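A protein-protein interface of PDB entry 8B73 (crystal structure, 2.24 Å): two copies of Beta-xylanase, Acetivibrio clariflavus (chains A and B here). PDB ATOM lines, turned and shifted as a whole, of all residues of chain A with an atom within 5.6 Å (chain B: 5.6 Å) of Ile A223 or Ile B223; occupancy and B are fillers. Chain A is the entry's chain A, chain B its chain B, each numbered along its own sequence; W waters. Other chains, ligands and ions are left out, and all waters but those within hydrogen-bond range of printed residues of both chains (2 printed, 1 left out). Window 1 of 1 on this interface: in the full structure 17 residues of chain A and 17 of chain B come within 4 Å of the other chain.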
ATOM      1  N   VAL A 169      17.146  12.054 -37.354  1.00  0.00           N
ATOM      2  CA  VAL A 169      18.161  12.570 -36.442  1.00  0.00           C
ATOM      3  C   VAL A 169      19.064  13.571 -37.174  1.00  0.00           C
ATOM      4  O   VAL A 169      19.332  14.652 -36.650  1.00  0.00           O
ATOM      5  CB  VAL A 169      18.975  11.441 -35.775  1.00  0.00           C
ATOM      6  CG1 VAL A 169      20.122  11.986 -34.935  1.00  0.00           C
ATOM      7  CG2 VAL A 169      18.092  10.536 -34.928  1.00  0.00           C
ATOM      8  N   ARG A 190      11.962  18.353 -35.777  1.00  0.00           N
ATOM      9  CA  ARG A 190      11.869  16.930 -36.070  1.00  0.00           C
ATOM     10  C   ARG A 190      10.505  16.400 -35.633  1.00  0.00           C
ATOM     11  O   ARG A 190       9.850  15.673 -36.381  1.00  0.00           O
ATOM     12  CB  ARG A 190      13.030  16.170 -35.406  1.00  0.00           C
ATOM     13  CG  ARG A 190      14.356  16.282 -36.152  1.00  0.00           C
ATOM     14  CD  ARG A 190      15.566  15.639 -35.487  1.00  0.00           C
ATOM     15  NE  ARG A 190      16.189  16.591 -34.587  1.00  0.00           N
ATOM     16  CZ  ARG A 190      17.445  17.025 -34.639  1.00  0.00           C
ATOM     17  NH1 ARG A 190      18.364  16.404 -35.353  1.00  0.00           N
ATOM     18  NH2 ARG A 190      17.790  18.067 -33.907  1.00  0.00           N
ATOM     19  N   ILE A 191      10.070  16.773 -34.424  1.00  0.00           N
ATOM     20  CA  ILE A 191       8.928  16.116 -33.811  1.00  0.00           C
ATOM     21  C   ILE A 191       7.629  16.542 -34.503  1.00  0.00           C
ATOM     22  O   ILE A 191       6.794  15.688 -34.808  1.00  0.00           O
ATOM     23  CB  ILE A 191       8.925  16.319 -32.282  1.00  0.00           C
ATOM     24  CG1 ILE A 191      10.020  15.460 -31.640  1.00  0.00           C
ATOM     25  CG2 ILE A 191       7.552  16.023 -31.691  1.00  0.00           C
ATOM     26  CD1 ILE A 191      10.145  15.596 -30.148  1.00  0.00           C
ATOM     27  N   GLU A 219      21.845   7.104 -28.567  1.00  0.00           N
ATOM     28  CA  GLU A 219      20.707   7.496 -27.750  1.00  0.00           C
ATOM     29  C   GLU A 219      19.913   8.636 -28.394  1.00  0.00           C
ATOM     30  O   GLU A 219      18.801   8.911 -27.964  1.00  0.00           O
ATOM     31  CB  GLU A 219      21.120   7.846 -26.316  1.00  0.00           C
ATOM     32  CG  GLU A 219      22.135   8.970 -26.185  1.00  0.00           C
ATOM     33  CD  GLU A 219      23.599   8.550 -26.195  1.00  0.00           C
ATOM     34  OE1 GLU A 219      23.876   7.365 -26.480  1.00  0.00           O
ATOM     35  OE2 GLU A 219      24.461   9.409 -25.910  1.00  0.00           O
ATOM     36  N   SER A 220      20.451   9.293 -29.430  1.00  0.00           N
ATOM     37  CA  SER A 220      19.717  10.370 -30.080  1.00  0.00           C
ATOM     38  C   SER A 220      18.476   9.828 -30.798  1.00  0.00           C
ATOM     39  O   SER A 220      17.460  10.516 -30.850  1.00  0.00           O
ATOM     40  CB  SER A 220      20.605  11.200 -30.988  1.00  0.00           C
ATOM     41  OG  SER A 220      21.267  10.395 -31.942  1.00  0.00           O
ATOM     42  N   TYR A 221      18.532   8.591 -31.314  1.00  0.00           N
ATOM     43  CA  TYR A 221      17.392   8.012 -32.015  1.00  0.00           C
ATOM     44  C   TYR A 221      16.342   7.522 -31.017  1.00  0.00           C
ATOM     45  O   TYR A 221      15.154   7.752 -31.227  1.00  0.00           O
ATOM     46  CB  TYR A 221      17.840   6.903 -32.970  1.00  0.00           C
ATOM     47  CG  TYR A 221      16.777   6.314 -33.872  1.00  0.00           C
ATOM     48  CD1 TYR A 221      15.783   7.095 -34.443  1.00  0.00           C
ATOM     49  CD2 TYR A 221      16.799   4.965 -34.205  1.00  0.00           C
ATOM     50  CE1 TYR A 221      14.828   6.552 -35.290  1.00  0.00           C
ATOM     51  CE2 TYR A 221      15.862   4.405 -35.058  1.00  0.00           C
ATOM     52  CZ  TYR A 221      14.870   5.202 -35.604  1.00  0.00           C
ATOM     53  OH  TYR A 221      13.937   4.647 -36.441  1.00  0.00           O
ATOM     54  N   ASP A 222      16.766   6.869 -29.928  1.00  0.00           N
ATOM     55  CA  ASP A 222      15.812   6.372 -28.945  1.00  0.00           C
ATOM     56  C   ASP A 222      15.206   7.544 -28.165  1.00  0.00           C
ATOM     57  O   ASP A 222      14.040   7.479 -27.775  1.00  0.00           O
ATOM     58  CB  ASP A 222      16.399   5.242 -28.082  1.00  0.00           C
ATOM     59  CG  ASP A 222      17.354   5.630 -26.962  1.00  0.00           C
ATOM     60  OD1 ASP A 222      16.914   6.265 -25.989  1.00  0.00           O
ATOM     61  OD2 ASP A 222      18.519   5.230 -27.035  1.00  0.00           O
ATOM     62  N   ILE A 223      15.965   8.631 -27.970  1.00  0.00           N
ATOM     63  CA  ILE A 223      15.412   9.818 -27.335  1.00  0.00           C
ATOM     64  C   ILE A 223      14.369  10.450 -28.258  1.00  0.00           C
ATOM     65  O   ILE A 223      13.299  10.828 -27.794  1.00  0.00           O
ATOM     66  CB  ILE A 223      16.514  10.809 -26.910  1.00  0.00           C
ATOM     67  CG1 ILE A 223      17.307  10.268 -25.719  1.00  0.00           C
ATOM     68  CG2 ILE A 223      15.927  12.180 -26.596  1.00  0.00           C
ATOM     69  CD1 ILE A 223      18.590  11.017 -25.432  1.00  0.00           C
ATOM     70  N   LEU A 224      14.670  10.546 -29.562  1.00  0.00           N
ATOM     71  CA  LEU A 224      13.716  11.060 -30.536  1.00  0.00           C
ATOM     72  C   LEU A 224      12.411  10.269 -30.477  1.00  0.00           C
ATOM     73  O   LEU A 224      11.335  10.858 -30.427  1.00  0.00           O
ATOM     74  CB  LEU A 224      14.312  10.982 -31.946  1.00  0.00           C
ATOM     75  CG  LEU A 224      13.383  11.437 -33.072  1.00  0.00           C
ATOM     76  CD1 LEU A 224      13.073  12.923 -32.951  1.00  0.00           C
ATOM     77  CD2 LEU A 224      13.987  11.133 -34.434  1.00  0.00           C
ATOM     78  N   ILE A 225      12.521   8.935 -30.502  1.00  0.00           N
ATOM     79  CA  ILE A 225      11.358   8.060 -30.505  1.00  0.00           C
ATOM     80  C   ILE A 225      10.545   8.257 -29.228  1.00  0.00           C
ATOM     81  O   ILE A 225       9.323   8.285 -29.289  1.00  0.00           O
ATOM     82  CB  ILE A 225      11.783   6.592 -30.702  1.00  0.00           C
ATOM     83  CG1 ILE A 225      12.292   6.362 -32.124  1.00  0.00           C
ATOM     84  CG2 ILE A 225      10.649   5.633 -30.355  1.00  0.00           C
ATOM     85  CD1 ILE A 225      12.985   5.035 -32.304  1.00  0.00           C
ATOM     86  N   GLU A 226      11.221   8.394 -28.081  1.00  0.00           N
ATOM     87  CA  GLU A 226      10.544   8.625 -26.811  1.00  0.00           C
ATOM     88  C   GLU A 226       9.757   9.935 -26.862  1.00  0.00           C
ATOM     89  O   GLU A 226       8.634   9.994 -26.371  1.00  0.00           O
ATOM     90  CB  GLU A 226      11.542   8.641 -25.653  1.00  0.00           C
ATOM     91  CG  GLU A 226      10.886   8.584 -24.287  1.00  0.00           C
ATOM     92  CD  GLU A 226      11.855   8.581 -23.115  1.00  0.00           C
ATOM     93  OE1 GLU A 226      12.905   7.905 -23.212  1.00  0.00           O
ATOM     94  OE2 GLU A 226      11.543   9.226 -22.095  1.00  0.00           O
ATOM     95  N   GLY A 227      10.354  10.977 -27.454  1.00  0.00           N
ATOM     96  CA  GLY A 227       9.696  12.264 -27.628  1.00  0.00           C
ATOM     97  C   GLY A 227       8.479  12.179 -28.549  1.00  0.00           C
ATOM     98  O   GLY A 227       7.452  12.796 -28.274  1.00  0.00           O
ATOM     99  N   LEU A 228       8.601  11.420 -29.641  1.00  0.00           N
ATOM    100  CA  LEU A 228       7.504  11.230 -30.576  1.00  0.00           C
ATOM    101  C   LEU A 228       6.326  10.537 -29.888  1.00  0.00           C
ATOM    102  O   LEU A 228       5.183  10.978 -30.023  1.00  0.00           O
ATOM    103  CB  LEU A 228       7.993  10.407 -31.773  1.00  0.00           C
ATOM    104  CG  LEU A 228       9.033  11.081 -32.668  1.00  0.00           C
ATOM    105  CD1 LEU A 228       9.571  10.091 -33.682  1.00  0.00           C
ATOM    106  CD2 LEU A 228       8.465  12.306 -33.372  1.00  0.00           C
ATOM    107  N   ARG A 263      12.489  -1.117 -25.144  1.00  0.00           N
ATOM    108  CA  ARG A 263      11.796  -0.565 -23.996  1.00  0.00           C
ATOM    109  C   ARG A 263      10.434  -0.001 -24.418  1.00  0.00           C
ATOM    110  O   ARG A 263       9.548   0.123 -23.579  1.00  0.00           O
ATOM    111  CB  ARG A 263      12.672   0.476 -23.283  1.00  0.00           C
ATOM    112  CG  ARG A 263      12.870   1.796 -24.018  1.00  0.00           C
ATOM    113  CD  ARG A 263      13.329   2.868 -23.050  1.00  0.00           C
ATOM    114  NE  ARG A 263      13.413   4.208 -23.623  1.00  0.00           N
ATOM    115  CZ  ARG A 263      14.446   4.671 -24.314  1.00  0.00           C
ATOM    116  NH1 ARG A 263      15.494   3.895 -24.525  1.00  0.00           N
ATOM    117  NH2 ARG A 263      14.431   5.909 -24.779  1.00  0.00           N
ATOM    118  N   PHE A 264      10.270   0.318 -25.712  1.00  0.00           N
ATOM    119  CA  PHE A 264       9.042   0.898 -26.236  1.00  0.00           C
ATOM    120  C   PHE A 264       7.972  -0.168 -26.478  1.00  0.00           C
ATOM    121  O   PHE A 264       6.810   0.172 -26.679  1.00  0.00           O
ATOM    122  CB  PHE A 264       9.331   1.660 -27.531  1.00  0.00           C
ATOM    123  CG  PHE A 264      10.355   2.760 -27.386  1.00  0.00           C
ATOM    124  CD1 PHE A 264      10.122   3.841 -26.547  1.00  0.00           C
ATOM    125  CD2 PHE A 264      11.556   2.711 -28.077  1.00  0.00           C
ATOM    126  CE1 PHE A 264      11.064   4.853 -26.413  1.00  0.00           C
ATOM    127  CE2 PHE A 264      12.498   3.721 -27.940  1.00  0.00           C
ATOM    128  CZ  PHE A 264      12.251   4.787 -27.106  1.00  0.00           C
ATOM    129  N   VAL B 169      20.702  12.969 -20.463  1.00  0.00           N
ATOM    130  CA  VAL B 169      21.041  12.177 -21.639  1.00  0.00           C
ATOM    131  C   VAL B 169      21.706  10.864 -21.211  1.00  0.00           C
ATOM    132  O   VAL B 169      21.336   9.805 -21.711  1.00  0.00           O
ATOM    133  CB  VAL B 169      21.912  12.961 -22.641  1.00  0.00           C
ATOM    134  CG1 VAL B 169      22.382  12.085 -23.795  1.00  0.00           C
ATOM    135  CG2 VAL B 169      21.191  14.185 -23.183  1.00  0.00           C
ATOM    136  N   ARG B 190      13.378   9.164 -19.576  1.00  0.00           N
ATOM    137  CA  ARG B 190      13.915  10.498 -19.376  1.00  0.00           C
ATOM    138  C   ARG B 190      12.777  11.513 -19.343  1.00  0.00           C
ATOM    139  O   ARG B 190      12.748  12.378 -18.470  1.00  0.00           O
ATOM    140  CB  ARG B 190      14.948  10.828 -20.466  1.00  0.00           C
ATOM    141  CG  ARG B 190      16.314  10.194 -20.237  1.00  0.00           C
ATOM    142  CD  ARG B 190      17.340  10.384 -21.347  1.00  0.00           C
ATOM    143  NE  ARG B 190      17.176   9.338 -22.337  1.00  0.00           N
ATOM    144  CZ  ARG B 190      18.097   8.467 -22.724  1.00  0.00           C
ATOM    145  NH1 ARG B 190      19.376   8.643 -22.451  1.00  0.00           N
ATOM    146  NH2 ARG B 190      17.716   7.434 -23.450  1.00  0.00           N
ATOM    147  N   ILE B 191      11.827  11.397 -20.276  1.00  0.00           N
ATOM    148  CA  ILE B 191      10.851  12.457 -20.476  1.00  0.00           C
ATOM    149  C   ILE B 191       9.839  12.485 -19.328  1.00  0.00           C
ATOM    150  O   ILE B 191       9.555  13.560 -18.802  1.00  0.00           O
ATOM    151  CB  ILE B 191      10.210  12.366 -21.877  1.00  0.00           C
ATOM    152  CG1 ILE B 191      11.219  12.816 -22.939  1.00  0.00           C
ATOM    153  CG2 ILE B 191       8.922  13.177 -21.946  1.00  0.00           C
ATOM    154  CD1 ILE B 191      10.729  12.710 -24.353  1.00  0.00           C
ATOM    155  N   GLU B 219      23.335  16.462 -30.677  1.00  0.00           N
ATOM    156  CA  GLU B 219      21.921  16.586 -30.996  1.00  0.00           C
ATOM    157  C   GLU B 219      21.053  15.755 -30.047  1.00  0.00           C
ATOM    158  O   GLU B 219      19.839  15.944 -30.024  1.00  0.00           O
ATOM    159  CB  GLU B 219      21.626  16.251 -32.462  1.00  0.00           C
ATOM    160  CG  GLU B 219      22.021  14.850 -32.899  1.00  0.00           C
ATOM    161  CD  GLU B 219      23.428  14.691 -33.452  1.00  0.00           C
ATOM    162  OE1 GLU B 219      24.230  15.642 -33.346  1.00  0.00           O
ATOM    163  OE2 GLU B 219      23.708  13.616 -34.013  1.00  0.00           O
ATOM    164  N   SER B 220      21.651  14.865 -29.241  1.00  0.00           N
ATOM    165  CA  SER B 220      20.866  14.094 -28.285  1.00  0.00           C
ATOM    166  C   SER B 220      20.255  14.998 -27.210  1.00  0.00           C
ATOM    167  O   SER B 220      19.153  14.724 -26.745  1.00  0.00           O
ATOM    168  CB  SER B 220      21.653  12.943 -27.685  1.00  0.00           C
ATOM    169  OG  SER B 220      22.857  13.394 -27.092  1.00  0.00           O
ATOM    170  N   TYR B 221      20.942  16.090 -26.839  1.00  0.00           N
ATOM    171  CA  TYR B 221      20.443  16.989 -25.807  1.00  0.00           C
ATOM    172  C   TYR B 221      19.355  17.897 -26.382  1.00  0.00           C
ATOM    173  O   TYR B 221      18.327  18.096 -25.743  1.00  0.00           O
ATOM    174  CB  TYR B 221      21.589  17.780 -25.163  1.00  0.00           C
ATOM    175  CG  TYR B 221      21.230  18.650 -23.977  1.00  0.00           C
ATOM    176  CD1 TYR B 221      20.291  18.258 -23.034  1.00  0.00           C
ATOM    177  CD2 TYR B 221      21.868  19.864 -23.771  1.00  0.00           C
ATOM    178  CE1 TYR B 221      19.980  19.053 -21.940  1.00  0.00           C
ATOM    179  CE2 TYR B 221      21.579  20.666 -22.678  1.00  0.00           C
ATOM    180  CZ  TYR B 221      20.632  20.258 -21.757  1.00  0.00           C
ATOM    181  OH  TYR B 221      20.342  21.050 -20.677  1.00  0.00           O
ATOM    182  N   ASP B 222      19.563  18.436 -27.589  1.00  0.00           N
ATOM    183  CA  ASP B 222      18.565  19.317 -28.186  1.00  0.00           C
ATOM    184  C   ASP B 222      17.336  18.507 -28.621  1.00  0.00           C
ATOM    185  O   ASP B 222      16.216  19.015 -28.574  1.00  0.00           O
ATOM    186  CB  ASP B 222      19.171  20.220 -29.272  1.00  0.00           C
ATOM    187  CG  ASP B 222      19.460  19.600 -30.630  1.00  0.00           C
ATOM    188  OD1 ASP B 222      18.503  19.237 -31.336  1.00  0.00           O
ATOM    189  OD2 ASP B 222      20.637  19.555 -30.998  1.00  0.00           O
ATOM    190  N   ILE B 223      17.519  17.240 -29.007  1.00  0.00           N
ATOM    191  CA  ILE B 223      16.377  16.389 -29.315  1.00  0.00           C
ATOM    192  C   ILE B 223      15.584  16.106 -28.036  1.00  0.00           C
ATOM    193  O   ILE B 223      14.358  16.174 -28.055  1.00  0.00           O
ATOM    194  CB  ILE B 223      16.808  15.103 -30.051  1.00  0.00           C
ATOM    195  CG1 ILE B 223      17.231  15.421 -31.489  1.00  0.00           C
ATOM    196  CG2 ILE B 223      15.706  14.053 -30.018  1.00  0.00           C
ATOM    197  CD1 ILE B 223      17.961  14.296 -32.187  1.00  0.00           C
ATOM    198  N   LEU B 224      16.279  15.816 -26.928  1.00  0.00           N
ATOM    199  CA  LEU B 224      15.627  15.606 -25.645  1.00  0.00           C
ATOM    200  C   LEU B 224      14.778  16.823 -25.275  1.00  0.00           C
ATOM    201  O   LEU B 224      13.619  16.675 -24.889  1.00  0.00           O
ATOM    202  CB  LEU B 224      16.682  15.342 -24.564  1.00  0.00           C
ATOM    203  CG  LEU B 224      16.146  15.220 -23.138  1.00  0.00           C
ATOM    204  CD1 LEU B 224      15.267  13.988 -22.993  1.00  0.00           C
ATOM    205  CD2 LEU B 224      17.282  15.196 -22.124  1.00  0.00           C
ATOM    206  N   ILE B 225      15.372  18.018 -25.391  1.00  0.00           N
ATOM    207  CA  ILE B 225      14.697  19.256 -25.036  1.00  0.00           C
ATOM    208  C   ILE B 225      13.457  19.454 -25.905  1.00  0.00           C
ATOM    209  O   ILE B 225      12.419  19.869 -25.395  1.00  0.00           O
ATOM    210  CB  ILE B 225      15.670  20.449 -25.116  1.00  0.00           C
ATOM    211  CG1 ILE B 225      16.703  20.381 -23.987  1.00  0.00           C
ATOM    212  CG2 ILE B 225      14.917  21.772 -25.103  1.00  0.00           C
ATOM    213  CD1 ILE B 225      17.863  21.324 -24.175  1.00  0.00           C
ATOM    214  N   GLU B 226      13.567  19.162 -27.207  1.00  0.00           N
ATOM    215  CA  GLU B 226      12.440  19.291 -28.117  1.00  0.00           C
ATOM    216  C   GLU B 226      11.306  18.363 -27.682  1.00  0.00           C
ATOM    217  O   GLU B 226      10.141  18.752 -27.728  1.00  0.00           O
ATOM    218  CB  GLU B 226      12.865  18.990 -29.555  1.00  0.00           C
ATOM    219  CG  GLU B 226      11.816  19.359 -30.592  1.00  0.00           C
ATOM    220  CD  GLU B 226      12.238  19.121 -32.032  1.00  0.00           C
ATOM    221  OE1 GLU B 226      13.409  19.403 -32.354  1.00  0.00           O
ATOM    222  OE2 GLU B 226      11.390  18.682 -32.839  1.00  0.00           O
ATOM    223  N   GLY B 227      11.652  17.135 -27.272  1.00  0.00           N
ATOM    224  CA  GLY B 227      10.674  16.170 -26.787  1.00  0.00           C
ATOM    225  C   GLY B 227       9.996  16.618 -25.493  1.00  0.00           C
ATOM    226  O   GLY B 227       8.792  16.445 -25.329  1.00  0.00           O
ATOM    227  N   LEU B 228      10.778  17.199 -24.577  1.00  0.00           N
ATOM    228  CA  LEU B 228      10.252  17.719 -23.324  1.00  0.00           C
ATOM    229  C   LEU B 228       9.242  18.837 -23.591  1.00  0.00           C
ATOM    230  O   LEU B 228       8.153  18.840 -23.020  1.00  0.00           O
ATOM    231  CB  LEU B 228      11.414  18.218 -22.456  1.00  0.00           C
ATOM    232  CG  LEU B 228      12.380  17.146 -21.949  1.00  0.00           C
ATOM    233  CD1 LEU B 228      13.590  17.775 -21.279  1.00  0.00           C
ATOM    234  CD2 LEU B 228      11.692  16.196 -20.990  1.00  0.00           C
ATOM    235  N   ARG B 263      17.078  27.707 -31.094  1.00  0.00           N
ATOM    236  CA  ARG B 263      15.863  27.534 -31.871  1.00  0.00           C
ATOM    237  C   ARG B 263      14.644  27.472 -30.945  1.00  0.00           C
ATOM    238  O   ARG B 263      13.533  27.737 -31.394  1.00  0.00           O
ATOM    239  CB  ARG B 263      15.988  26.311 -32.786  1.00  0.00           C
ATOM    240  CG  ARG B 263      15.958  24.959 -32.084  1.00  0.00           C
ATOM    241  CD  ARG B 263      15.632  23.858 -33.078  1.00  0.00           C
ATOM    242  NE  ARG B 263      15.401  22.556 -32.469  1.00  0.00           N
ATOM    243  CZ  ARG B 263      16.359  21.700 -32.141  1.00  0.00           C
ATOM    244  NH1 ARG B 263      17.620  22.022 -32.357  1.00  0.00           N
ATOM    245  NH2 ARG B 263      16.052  20.526 -31.610  1.00  0.00           N
ATOM    246  N   PHE B 264      14.854  27.148 -29.659  1.00  0.00           N
ATOM    247  CA  PHE B 264      13.768  27.018 -28.694  1.00  0.00           C
ATOM    248  C   PHE B 264      13.329  28.372 -28.146  1.00  0.00           C
ATOM    249  O   PHE B 264      12.288  28.451 -27.503  1.00  0.00           O
ATOM    250  CB  PHE B 264      14.191  26.118 -27.533  1.00  0.00           C
ATOM    251  CG  PHE B 264      14.619  24.738 -27.954  1.00  0.00           C
ATOM    252  CD1 PHE B 264      13.723  23.882 -28.575  1.00  0.00           C
ATOM    253  CD2 PHE B 264      15.922  24.306 -27.748  1.00  0.00           C
ATOM    254  CE1 PHE B 264      14.119  22.618 -28.977  1.00  0.00           C
ATOM    255  CE2 PHE B 264      16.315  23.041 -28.155  1.00  0.00           C
ATOM    256  CZ  PHE B 264      15.414  22.201 -28.766  1.00  0.00           C
HETATM  257  O   HOH W   1      24.617  11.468 -27.316  1.00  0.00           O
HETATM  258  O   HOH W   2      19.129   5.446 -24.181  1.00  0.00           O
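NH2 of Arg A190 is in salt-bridge range of OD1 of Asp B222, 2.9 Å away.
N of Arg A190 lies within hydrogen-bond range of OE2 of Glu B226 (3.0 Å).
The side-chain carboxylate (OE2) of Glu B226 is in hydrogen-bond range of the backbone NH (N) of Ile A191 (2.8 Å).
The side-chain carboxylate (OD1) of Asp A222 is in salt-bridge range of the guanidinium group (NH2) of Arg B190 (2.9 Å).
OE2 of Glu A226 sits at hydrogen-bond distance from N of Arg B190, at 3.1 Å.
OE2 of Glu A226 is in hydrogen-bond range of N of Ile B191 (2.8 Å).
The side-chain carboxylate (OD1) of Asp A222 is in salt-bridge range of the guanidinium group (NH2) of Arg A263, at 2.8 Å.
The side-chain carboxylate (OE1) of Glu A226 is in salt-bridge range of the guanidinium group (NH2) of Arg A263, 3.0 Å away.
OD1 of Asp B222 lies within salt-bridge range of NH2 of Arg B263, at 2.8 Å.
The guanidinium group (NH2) of Arg B263 lies within salt-bridge range of the side-chain carboxylate (OE1) of Glu B226 (3.0 Å).
CG1 of Val A169 touches CG of Glu B219, 3.99 Å away.
Arg A190 touches Ile B223.
Glu A219 touches Val B169 (CG to CG1, 3.9 Å).
Ser A220 touches Ser B220 (CB to CB, 3.9 Å).
NE of Arg B190 touches CG1 of Ile A223, 3.5 Å away.
CD1 of Ile A223 touches O of Ser B220 (3.97 Å).
Ile B223 touches Ile A223 (CG2 to CG2, 3.9 Å).
CA of Leu A224 touches CG2 of Ile B223 (3.6 Å).
CA of Gly A227 touches CD1 of Ile B191 (3.5 Å).
Arg A263 touches Arg B190 (NH2 to NH2, 3.9 Å).
Of chain B, only Arg B190 (3.5 Å), Ser B220 (3.97 Å), Ile B223 (3.9 Å) and Leu B224 (3.6 Å) come within 4 Å of Ile A223.
Of the printed residues of chain B, Glu A226 touches Arg B190 and Ile B191.
Printed residues of chain A within 4 Å of Val B169: Glu A219.
Of the printed residues of chain A, Ile B191 touches Glu A226 and Gly A227.
Of the printed residues of chain A, Glu B219 touches Val A169 (3.99 Å).
Of chain A, only Arg A190, Ile A223 and Leu A224 come within 4 Å of Ile B223.
Of the printed residues of chain A, Leu B224 touches Ile A223 (3.6 Å).
The nearest residue of chain B that does not touch Ile A223 is Val B169 (4.3 Å).
The nearest printed residue of chain A that does not touch Ile B191 is Ile A223 (4.7 Å).
Of the 15 printed residues of chain A, 11 touch a printed residue of chain B.
Along chain A the printed residues that touch a printed residue of chain B span positions 169 to 263.
Of the 15 printed residues of chain B, 11 touch a printed residue of chain A.
Hydrophobic or aromatic side chains of chain B within 4 Å of the printed part of chain A: Val B169, Ile B191, Ile B223 and Leu B224.
Among the printed residues, 19 pairs touch across the chains.
Among the printed residues, Asp or Glu carboxylates within 4 Å of a Lys or Arg side-chain nitrogen of the other chain: Arg A190 with Asp B222 (2.9 Å) and Asp A222 with Arg B190 (2.9 Å).
Arg A190 touches Asp B222, and with the chains exchanged Asp A222 touches Arg B190.
Ile A191 touches Gly B227, and with the chains exchanged Gly A227 touches Ile B191.
Ile B223 touches its own counterpart, Ile A223.
Ile A223 touches Leu B224, and with the chains exchanged Leu A224 touches Ile B223.
Positions printed for both chains: 169, 190, 191, 219, 220, 221, 222, 223, 224, 225, 226, 227, 228, 263 and 264.
Water W1 lies within hydrogen-bond range of OE2 of Glu A219 (2.5 Å) and OG of Ser B220 (2.6 Å).
Water W2 bridges NH2 of Arg B190 (2.5 Å) and OD2 of Asp A222 (2.9 Å).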
